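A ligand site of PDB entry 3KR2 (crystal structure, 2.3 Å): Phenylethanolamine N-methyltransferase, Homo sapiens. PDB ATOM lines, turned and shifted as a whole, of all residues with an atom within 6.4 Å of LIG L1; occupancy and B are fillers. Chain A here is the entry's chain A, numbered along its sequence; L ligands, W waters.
O of Tyr 35 sits at hydrogen-bond distance from ND2 of Asn 39.
The side-chain hydroxyl (OH) of Tyr 85 sits at hydrogen-bond distance from the side-chain hydroxyl (OH) of Tyr 40 (3.2 Å).
OD1 of Asn 39 lies within hydrogen-bond range of NH1 of Arg 44 (3.0 Å).
NH1 of Arg 44 is in salt-bridge range of OD2 of Asp 267.
O of Leu 262 is in hydrogen-bond range of NE of Arg 44 (2.8 Å).
N of Val 53 sits at hydrogen-bond distance from OH of Tyr 256, at 3.2 Å.
The side-chain hydroxyl (OH) of Tyr 35 sits at hydrogen-bond distance from a nitrogen (N1) of LIG L1 (2.7 Å).
OH of Tyr 40 sits at hydrogen-bond distance from N3 of LIG L1.
The side-chain hydroxyl of Tyr 35 sits at hydrogen-bond distance from an oxygen (O1) of LG2 L2, 2.6 Å away.
The side-chain hydroxyl (OH) of Tyr 40 sits at hydrogen-bond distance from an oxygen (O1) of LG2 L2 (2.5 Å).
O2 of LG2 L2 is in hydrogen-bond range of OH of Tyr 85, at 2.7 Å.
A nitrogen (N1) of LG2 L2 lies within hydrogen-bond range of the backbone carbonyl oxygen of Ala 181 (2.7 Å).
A fluorine (F1) of LIG L1 lies close to the side-chain sulfur (SD) of Met 258.
Residues that only touch LIG L1: Asn 39 (3.5 Å), Arg 44 (3.3 Å), Val 53 (3.6 Å), Lys 57 (3.4 Å) and Phe 182 (3.2 Å).
Hydrophobic or aromatic side chains within 4 Å of LIG L1: Tyr 35, Tyr 40, Val 53, Phe 182 and Met 258.
Of the 20 residues printed, 8 come within 4 Å of LIG L1.
Along chain A the residues within 4 Å of LIG L1 span positions 35 to 258.
The nearest printed residue that does not touch LIG L1 is Asp 267 (4.5 Å).
Water W1 bridges a nitrogen (N1) of LIG L1 (2.7 Å) and the side-chain carboxylate (OE2) of Glu 219 (3.5 Å).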
ATOM      1  N   TYR A  35       4.246  34.093   2.289  1.00  0.00           N
ATOM      2  CA  TYR A  35       4.822  33.098   3.204  1.00  0.00           C
ATOM      3  C   TYR A  35       4.689  31.692   2.619  1.00  0.00           C
ATOM      4  O   TYR A  35       5.668  30.981   2.455  1.00  0.00           O
ATOM      5  CB  TYR A  35       4.164  33.165   4.593  1.00  0.00           C
ATOM      6  CG  TYR A  35       4.647  32.093   5.554  1.00  0.00           C
ATOM      7  CD1 TYR A  35       5.891  32.180   6.166  1.00  0.00           C
ATOM      8  CD2 TYR A  35       3.850  30.991   5.853  1.00  0.00           C
ATOM      9  CE1 TYR A  35       6.329  31.204   7.046  1.00  0.00           C
ATOM     10  CE2 TYR A  35       4.280  30.006   6.743  1.00  0.00           C
ATOM     11  CZ  TYR A  35       5.527  30.124   7.327  1.00  0.00           C
ATOM     12  OH  TYR A  35       5.951  29.149   8.198  1.00  0.00           O
ATOM     13  N   ASN A  39       7.784  29.043   1.322  1.00  0.00           N
ATOM     14  CA  ASN A  39       8.129  27.860   2.100  1.00  0.00           C
ATOM     15  C   ASN A  39       7.409  26.557   1.707  1.00  0.00           C
ATOM     16  O   ASN A  39       7.842  25.468   2.083  1.00  0.00           O
ATOM     17  CB  ASN A  39       7.942  28.139   3.586  1.00  0.00           C
ATOM     18  CG  ASN A  39       8.824  29.276   4.064  1.00  0.00           C
ATOM     19  OD1 ASN A  39      10.037  29.112   4.233  1.00  0.00           O
ATOM     20  ND2 ASN A  39       8.220  30.445   4.271  1.00  0.00           N
ATOM     21  N   TYR A  40       6.319  26.692   0.970  1.00  0.00           N
ATOM     22  CA  TYR A  40       5.483  25.531   0.661  1.00  0.00           C
ATOM     23  C   TYR A  40       5.165  25.374  -0.831  1.00  0.00           C
ATOM     24  O   TYR A  40       4.271  24.611  -1.190  1.00  0.00           O
ATOM     25  CB  TYR A  40       4.211  25.567   1.518  1.00  0.00           C
ATOM     26  CG  TYR A  40       4.571  25.574   2.987  1.00  0.00           C
ATOM     27  CD1 TYR A  40       4.530  26.742   3.733  1.00  0.00           C
ATOM     28  CD2 TYR A  40       5.032  24.412   3.608  1.00  0.00           C
ATOM     29  CE1 TYR A  40       4.876  26.747   5.071  1.00  0.00           C
ATOM     30  CE2 TYR A  40       5.387  24.403   4.942  1.00  0.00           C
ATOM     31  CZ  TYR A  40       5.311  25.581   5.678  1.00  0.00           C
ATOM     32  OH  TYR A  40       5.674  25.601   6.998  1.00  0.00           O
ATOM     33  N   ARG A  44      11.040  24.094  -2.020  1.00  0.00           N
ATOM     34  CA  ARG A  44      10.840  23.528  -0.687  1.00  0.00           C
ATOM     35  C   ARG A  44       9.545  22.766  -0.612  1.00  0.00           C
ATOM     36  O   ARG A  44       9.395  21.864   0.212  1.00  0.00           O
ATOM     37  CB  ARG A  44      10.880  24.618   0.398  1.00  0.00           C
ATOM     38  CG  ARG A  44      12.190  25.348   0.524  1.00  0.00           C
ATOM     39  CD  ARG A  44      12.177  26.329   1.683  1.00  0.00           C
ATOM     40  NE  ARG A  44      13.509  26.853   1.952  1.00  0.00           N
ATOM     41  CZ  ARG A  44      13.799  27.697   2.927  1.00  0.00           C
ATOM     42  NH1 ARG A  44      12.838  28.114   3.765  1.00  0.00           N
ATOM     43  NH2 ARG A  44      15.056  28.122   3.076  1.00  0.00           N
ATOM     44  N   VAL A  53      12.936  18.724   2.776  1.00  0.00           N
ATOM     45  CA  VAL A  53      12.476  19.119   4.096  1.00  0.00           C
ATOM     46  C   VAL A  53      10.998  18.775   4.315  1.00  0.00           C
ATOM     47  O   VAL A  53      10.602  18.402   5.427  1.00  0.00           O
ATOM     48  CB  VAL A  53      12.728  20.631   4.368  1.00  0.00           C
ATOM     49  CG1 VAL A  53      12.022  21.512   3.297  1.00  0.00           C
ATOM     50  CG2 VAL A  53      12.289  21.017   5.785  1.00  0.00           C
ATOM     51  N   GLY A  54      10.186  18.920   3.275  1.00  0.00           N
ATOM     52  CA  GLY A  54       8.762  18.630   3.399  1.00  0.00           C
ATOM     53  C   GLY A  54       8.528  17.161   3.770  1.00  0.00           C
ATOM     54  O   GLY A  54       7.820  16.870   4.733  1.00  0.00           O
ATOM     55  N   LYS A  57       9.694  16.423   7.378  1.00  0.00           N
ATOM     56  CA  LYS A  57       8.706  16.865   8.356  1.00  0.00           C
ATOM     57  C   LYS A  57       7.515  15.918   8.444  1.00  0.00           C
ATOM     58  O   LYS A  57       7.177  15.436   9.547  1.00  0.00           O
ATOM     59  CB  LYS A  57       8.229  18.286   8.038  1.00  0.00           C
ATOM     60  CG  LYS A  57       9.330  19.314   8.146  1.00  0.00           C
ATOM     61  CD  LYS A  57       8.806  20.741   8.031  1.00  0.00           C
ATOM     62  CE  LYS A  57       8.502  21.125   6.600  1.00  0.00           C
ATOM     63  NZ  LYS A  57       7.709  22.346   6.584  1.00  0.00           N
ATOM     64  N   TYR A  85      -0.443  21.341   6.890  1.00  0.00           N
ATOM     65  CA  TYR A  85       0.318  20.095   6.720  1.00  0.00           C
ATOM     66  C   TYR A  85       0.662  19.502   8.070  1.00  0.00           C
ATOM     67  O   TYR A  85       0.847  18.286   8.193  1.00  0.00           O
ATOM     68  CB  TYR A  85       1.610  20.370   5.957  1.00  0.00           C
ATOM     69  CG  TYR A  85       2.594  21.135   6.803  1.00  0.00           C
ATOM     70  CD1 TYR A  85       3.597  20.481   7.514  1.00  0.00           C
ATOM     71  CD2 TYR A  85       2.506  22.523   6.921  1.00  0.00           C
ATOM     72  CE1 TYR A  85       4.485  21.177   8.303  1.00  0.00           C
ATOM     73  CE2 TYR A  85       3.417  23.240   7.712  1.00  0.00           C
ATOM     74  CZ  TYR A  85       4.380  22.561   8.403  1.00  0.00           C
ATOM     75  OH  TYR A  85       5.275  23.237   9.180  1.00  0.00           O
ATOM     76  N   ALA A 181       4.507  24.478  14.891  1.00  0.00           N
ATOM     77  CA  ALA A 181       5.588  24.498  13.932  1.00  0.00           C
ATOM     78  C   ALA A 181       5.994  25.915  13.542  1.00  0.00           C
ATOM     79  O   ALA A 181       5.154  26.710  13.144  1.00  0.00           O
ATOM     80  CB  ALA A 181       5.198  23.683  12.694  1.00  0.00           C
ATOM     81  N   PHE A 182       7.285  26.211  13.681  1.00  0.00           N
ATOM     82  CA  PHE A 182       7.832  27.478  13.221  1.00  0.00           C
ATOM     83  C   PHE A 182       7.235  28.729  13.877  1.00  0.00           C
ATOM     84  O   PHE A 182       7.201  29.814  13.277  1.00  0.00           O
ATOM     85  CB  PHE A 182       7.723  27.545  11.706  1.00  0.00           C
ATOM     86  CG  PHE A 182       8.501  26.472  11.008  1.00  0.00           C
ATOM     87  CD1 PHE A 182       7.847  25.430  10.352  1.00  0.00           C
ATOM     88  CD2 PHE A 182       9.883  26.481  11.034  1.00  0.00           C
ATOM     89  CE1 PHE A 182       8.566  24.433   9.720  1.00  0.00           C
ATOM     90  CE2 PHE A 182      10.603  25.477  10.408  1.00  0.00           C
ATOM     91  CZ  PHE A 182       9.939  24.457   9.750  1.00  0.00           C
ATOM     92  N   GLU A 185      10.230  30.286  18.137  1.00  0.00           N
ATOM     93  CA  GLU A 185      11.495  30.865  17.737  1.00  0.00           C
ATOM     94  C   GLU A 185      11.279  32.061  16.806  1.00  0.00           C
ATOM     95  O   GLU A 185      12.122  32.946  16.693  1.00  0.00           O
ATOM     96  CB  GLU A 185      12.397  29.809  17.090  1.00  0.00           C
ATOM     97  CG  GLU A 185      12.070  29.487  15.621  1.00  0.00           C
ATOM     98  CD  GLU A 185      11.074  28.340  15.428  1.00  0.00           C
ATOM     99  OE1 GLU A 185      10.514  27.803  16.412  1.00  0.00           O
ATOM    100  OE2 GLU A 185      10.866  27.964  14.251  1.00  0.00           O
ATOM    101  N   ALA A 216      12.739  26.175  13.200  1.00  0.00           N
ATOM    102  CA  ALA A 216      13.976  26.491  12.490  1.00  0.00           C
ATOM    103  C   ALA A 216      15.181  26.502  13.429  1.00  0.00           C
ATOM    104  O   ALA A 216      15.092  26.992  14.561  1.00  0.00           O
ATOM    105  CB  ALA A 216      13.838  27.824  11.809  1.00  0.00           C
ATOM    106  N   GLU A 219      18.329  30.107  12.933  1.00  0.00           N
ATOM    107  CA  GLU A 219      17.763  31.069  11.988  1.00  0.00           C
ATOM    108  C   GLU A 219      17.683  32.444  12.664  1.00  0.00           C
ATOM    109  O   GLU A 219      17.392  32.521  13.856  1.00  0.00           O
ATOM    110  CB  GLU A 219      16.341  30.649  11.565  1.00  0.00           C
ATOM    111  CG  GLU A 219      15.674  31.658  10.629  1.00  0.00           C
ATOM    112  CD  GLU A 219      14.275  31.225  10.182  1.00  0.00           C
ATOM    113  OE1 GLU A 219      14.087  30.987   8.960  1.00  0.00           O
ATOM    114  OE2 GLU A 219      13.371  31.134  11.015  1.00  0.00           O
ATOM    115  N   TYR A 222      13.440  35.810   8.470  1.00  0.00           N
ATOM    116  CA  TYR A 222      12.752  35.284   7.295  1.00  0.00           C
ATOM    117  C   TYR A 222      11.778  36.338   6.789  1.00  0.00           C
ATOM    118  O   TYR A 222      11.322  37.201   7.551  1.00  0.00           O
ATOM    119  CB  TYR A 222      12.060  33.949   7.579  1.00  0.00           C
ATOM    120  CG  TYR A 222      10.776  34.056   8.365  1.00  0.00           C
ATOM    121  CD1 TYR A 222       9.553  34.035   7.716  1.00  0.00           C
ATOM    122  CD2 TYR A 222      10.776  34.190   9.759  1.00  0.00           C
ATOM    123  CE1 TYR A 222       8.364  34.129   8.409  1.00  0.00           C
ATOM    124  CE2 TYR A 222       9.573  34.284  10.471  1.00  0.00           C
ATOM    125  CZ  TYR A 222       8.378  34.251   9.781  1.00  0.00           C
ATOM    126  OH  TYR A 222       7.187  34.342  10.437  1.00  0.00           O
ATOM    127  N   TYR A 256      17.158  18.118  10.883  1.00  0.00           N
ATOM    128  CA  TYR A 256      17.292  18.080   9.440  1.00  0.00           C
ATOM    129  C   TYR A 256      18.213  19.217   9.066  1.00  0.00           C
ATOM    130  O   TYR A 256      17.914  20.363   9.333  1.00  0.00           O
ATOM    131  CB  TYR A 256      15.903  18.247   8.784  1.00  0.00           C
ATOM    132  CG  TYR A 256      15.960  18.353   7.285  1.00  0.00           C
ATOM    133  CD1 TYR A 256      15.993  17.205   6.484  1.00  0.00           C
ATOM    134  CD2 TYR A 256      15.969  19.595   6.642  1.00  0.00           C
ATOM    135  CE1 TYR A 256      16.045  17.294   5.097  1.00  0.00           C
ATOM    136  CE2 TYR A 256      16.016  19.698   5.273  1.00  0.00           C
ATOM    137  CZ  TYR A 256      16.056  18.540   4.492  1.00  0.00           C
ATOM    138  OH  TYR A 256      16.108  18.641   3.136  1.00  0.00           O
ATOM    139  N   MET A 258      19.796  21.733   6.376  1.00  0.00           N
ATOM    140  CA  MET A 258      19.212  22.333   5.189  1.00  0.00           C
ATOM    141  C   MET A 258      20.174  22.225   3.986  1.00  0.00           C
ATOM    142  O   MET A 258      21.220  22.877   3.960  1.00  0.00           O
ATOM    143  CB  MET A 258      18.837  23.794   5.486  1.00  0.00           C
ATOM    144  CG  MET A 258      17.700  24.383   4.632  1.00  0.00           C
ATOM    145  SD  MET A 258      16.043  23.662   4.885  1.00  0.00           S
ATOM    146  CE  MET A 258      15.580  24.377   6.451  1.00  0.00           C
ATOM    147  N   LEU A 262      18.029  24.088  -1.025  1.00  0.00           N
ATOM    148  CA  LEU A 262      16.824  24.577  -0.352  1.00  0.00           C
ATOM    149  C   LEU A 262      17.050  25.882   0.423  1.00  0.00           C
ATOM    150  O   LEU A 262      16.151  26.389   1.093  1.00  0.00           O
ATOM    151  CB  LEU A 262      16.203  23.505   0.528  1.00  0.00           C
ATOM    152  CG  LEU A 262      15.566  22.367  -0.257  1.00  0.00           C
ATOM    153  CD1 LEU A 262      14.780  21.459   0.651  1.00  0.00           C
ATOM    154  CD2 LEU A 262      14.684  22.893  -1.382  1.00  0.00           C
ATOM    155  N   ASP A 267      15.136  33.321   3.739  1.00  0.00           N
ATOM    156  CA  ASP A 267      15.524  33.304   5.136  1.00  0.00           C
ATOM    157  C   ASP A 267      16.958  32.863   5.231  1.00  0.00           C
ATOM    158  O   ASP A 267      17.673  32.838   4.225  1.00  0.00           O
ATOM    159  CB  ASP A 267      14.599  32.389   5.978  1.00  0.00           C
ATOM    160  CG  ASP A 267      14.567  30.934   5.481  1.00  0.00           C
ATOM    161  OD1 ASP A 267      15.630  30.381   5.081  1.00  0.00           O
ATOM    162  OD2 ASP A 267      13.450  30.344   5.507  1.00  0.00           O
ATOM    163  N   VAL A 269      17.661  30.115   7.581  1.00  0.00           N
ATOM    164  CA  VAL A 269      17.542  28.906   8.398  1.00  0.00           C
ATOM    165  C   VAL A 269      18.659  27.919   8.039  1.00  0.00           C
ATOM    166  O   VAL A 269      18.985  27.746   6.862  1.00  0.00           O
ATOM    167  CB  VAL A 269      16.156  28.266   8.195  1.00  0.00           C
ATOM    168  CG1 VAL A 269      15.883  28.126   6.712  1.00  0.00           C
ATOM    169  CG2 VAL A 269      16.057  26.917   8.893  1.00  0.00           C
ATOM    170  N   VAL A 272      16.244  22.257  10.507  1.00  0.00           N
ATOM    171  CA  VAL A 272      14.901  22.188  11.069  1.00  0.00           C
ATOM    172  C   VAL A 272      14.923  21.124  12.163  1.00  0.00           C
ATOM    173  O   VAL A 272      15.564  20.085  11.994  1.00  0.00           O
ATOM    174  CB  VAL A 272      13.854  21.783   9.975  1.00  0.00           C
ATOM    175  CG1 VAL A 272      12.525  21.372  10.608  1.00  0.00           C
ATOM    176  CG2 VAL A 272      13.637  22.908   8.954  1.00  0.00           C
HETATM  177  N1  LIG L   1       8.539  28.702   8.648  1.00  0.00           N
HETATM  178  F1  LIG L   1      12.899  24.656   4.808  1.00  0.00           F
HETATM  179  C1  LIG L   1      10.532  24.644   4.992  1.00  0.00           C
HETATM  180  C2  LIG L   1       9.369  25.170   5.535  1.00  0.00           C
HETATM  181  C3  LIG L   1      11.837  26.229   6.246  1.00  0.00           C
HETATM  182  N2  LIG L   1      10.442  27.732   7.645  1.00  0.00           N
HETATM  183  N3  LIG L   1       8.509  26.906   7.087  1.00  0.00           N
HETATM  184  C4  LIG L   1      11.766  25.174   5.347  1.00  0.00           C
HETATM  185  C5  LIG L   1       9.126  27.828   7.834  1.00  0.00           C
HETATM  186  C6  LIG L   1      10.671  26.748   6.781  1.00  0.00           C
HETATM  187  C7  LIG L   1       9.437  26.219   6.426  1.00  0.00           C
HETATM  188  N1  LG2 L   2       2.894  26.985  11.682  1.00  0.00           N
HETATM  189  C1  LG2 L   2       2.955  27.484  10.320  1.00  0.00           C
HETATM  190  C2  LG2 L   2       3.229  28.989  10.314  1.00  0.00           C
HETATM  191  C3  LG2 L   2       4.439  29.377  11.172  1.00  0.00           C
HETATM  192  S1  LG2 L   2       5.012  31.067  10.816  1.00  0.00           S
HETATM  193  C4  LG2 L   2       4.041  26.724   9.568  1.00  0.00           C
HETATM  194  O1  LG2 L   2       4.333  27.114   8.493  1.00  0.00           O
HETATM  195  O2  LG2 L   2       4.509  25.570  10.180  1.00  0.00           O
HETATM  196  C5  LG2 L   2       4.852  31.828  12.464  1.00  0.00           C
HETATM  197  C6  LG2 L   2       3.416  32.147  12.874  1.00  0.00           C
HETATM  198  O3  LG2 L   2       3.490  32.701  14.138  1.00  0.00           O
HETATM  199  C7  LG2 L   2       2.828  33.253  12.005  1.00  0.00           C
HETATM  200  O4  LG2 L   2       1.661  32.757  11.376  1.00  0.00           O
HETATM  201  C8  LG2 L   2       2.560  34.270  12.908  1.00  0.00           C
HETATM  202  O5  LG2 L   2       1.414  35.030  12.638  1.00  0.00           O
HETATM  203  C9  LG2 L   2       2.461  33.633  14.170  1.00  0.00           C
HETATM  204  N2  LG2 L   2       2.562  34.561  15.292  1.00  0.00           N
HETATM  205  C10 LG2 L   2       3.091  35.791  15.253  1.00  0.00           C
HETATM  206  N3  LG2 L   2       3.027  36.325  16.516  1.00  0.00           N
HETATM  207  C11 LG2 L   2       2.456  35.405  17.343  1.00  0.00           C
HETATM  208  C12 LG2 L   2       2.159  35.427  18.682  1.00  0.00           C
HETATM  209  N4  LG2 L   2       2.503  36.603  19.472  1.00  0.00           N
HETATM  210  N5  LG2 L   2       1.596  34.378  19.261  1.00  0.00           N
HETATM  211  C13 LG2 L   2       1.303  33.280  18.522  1.00  0.00           C
HETATM  212  N6  LG2 L   2       1.584  33.265  17.197  1.00  0.00           N
HETATM  213  C14 LG2 L   2       2.169  34.319  16.619  1.00  0.00           C
HETATM  214  O   HOH W   1      10.571  30.490   9.035  1.00  0.00           O
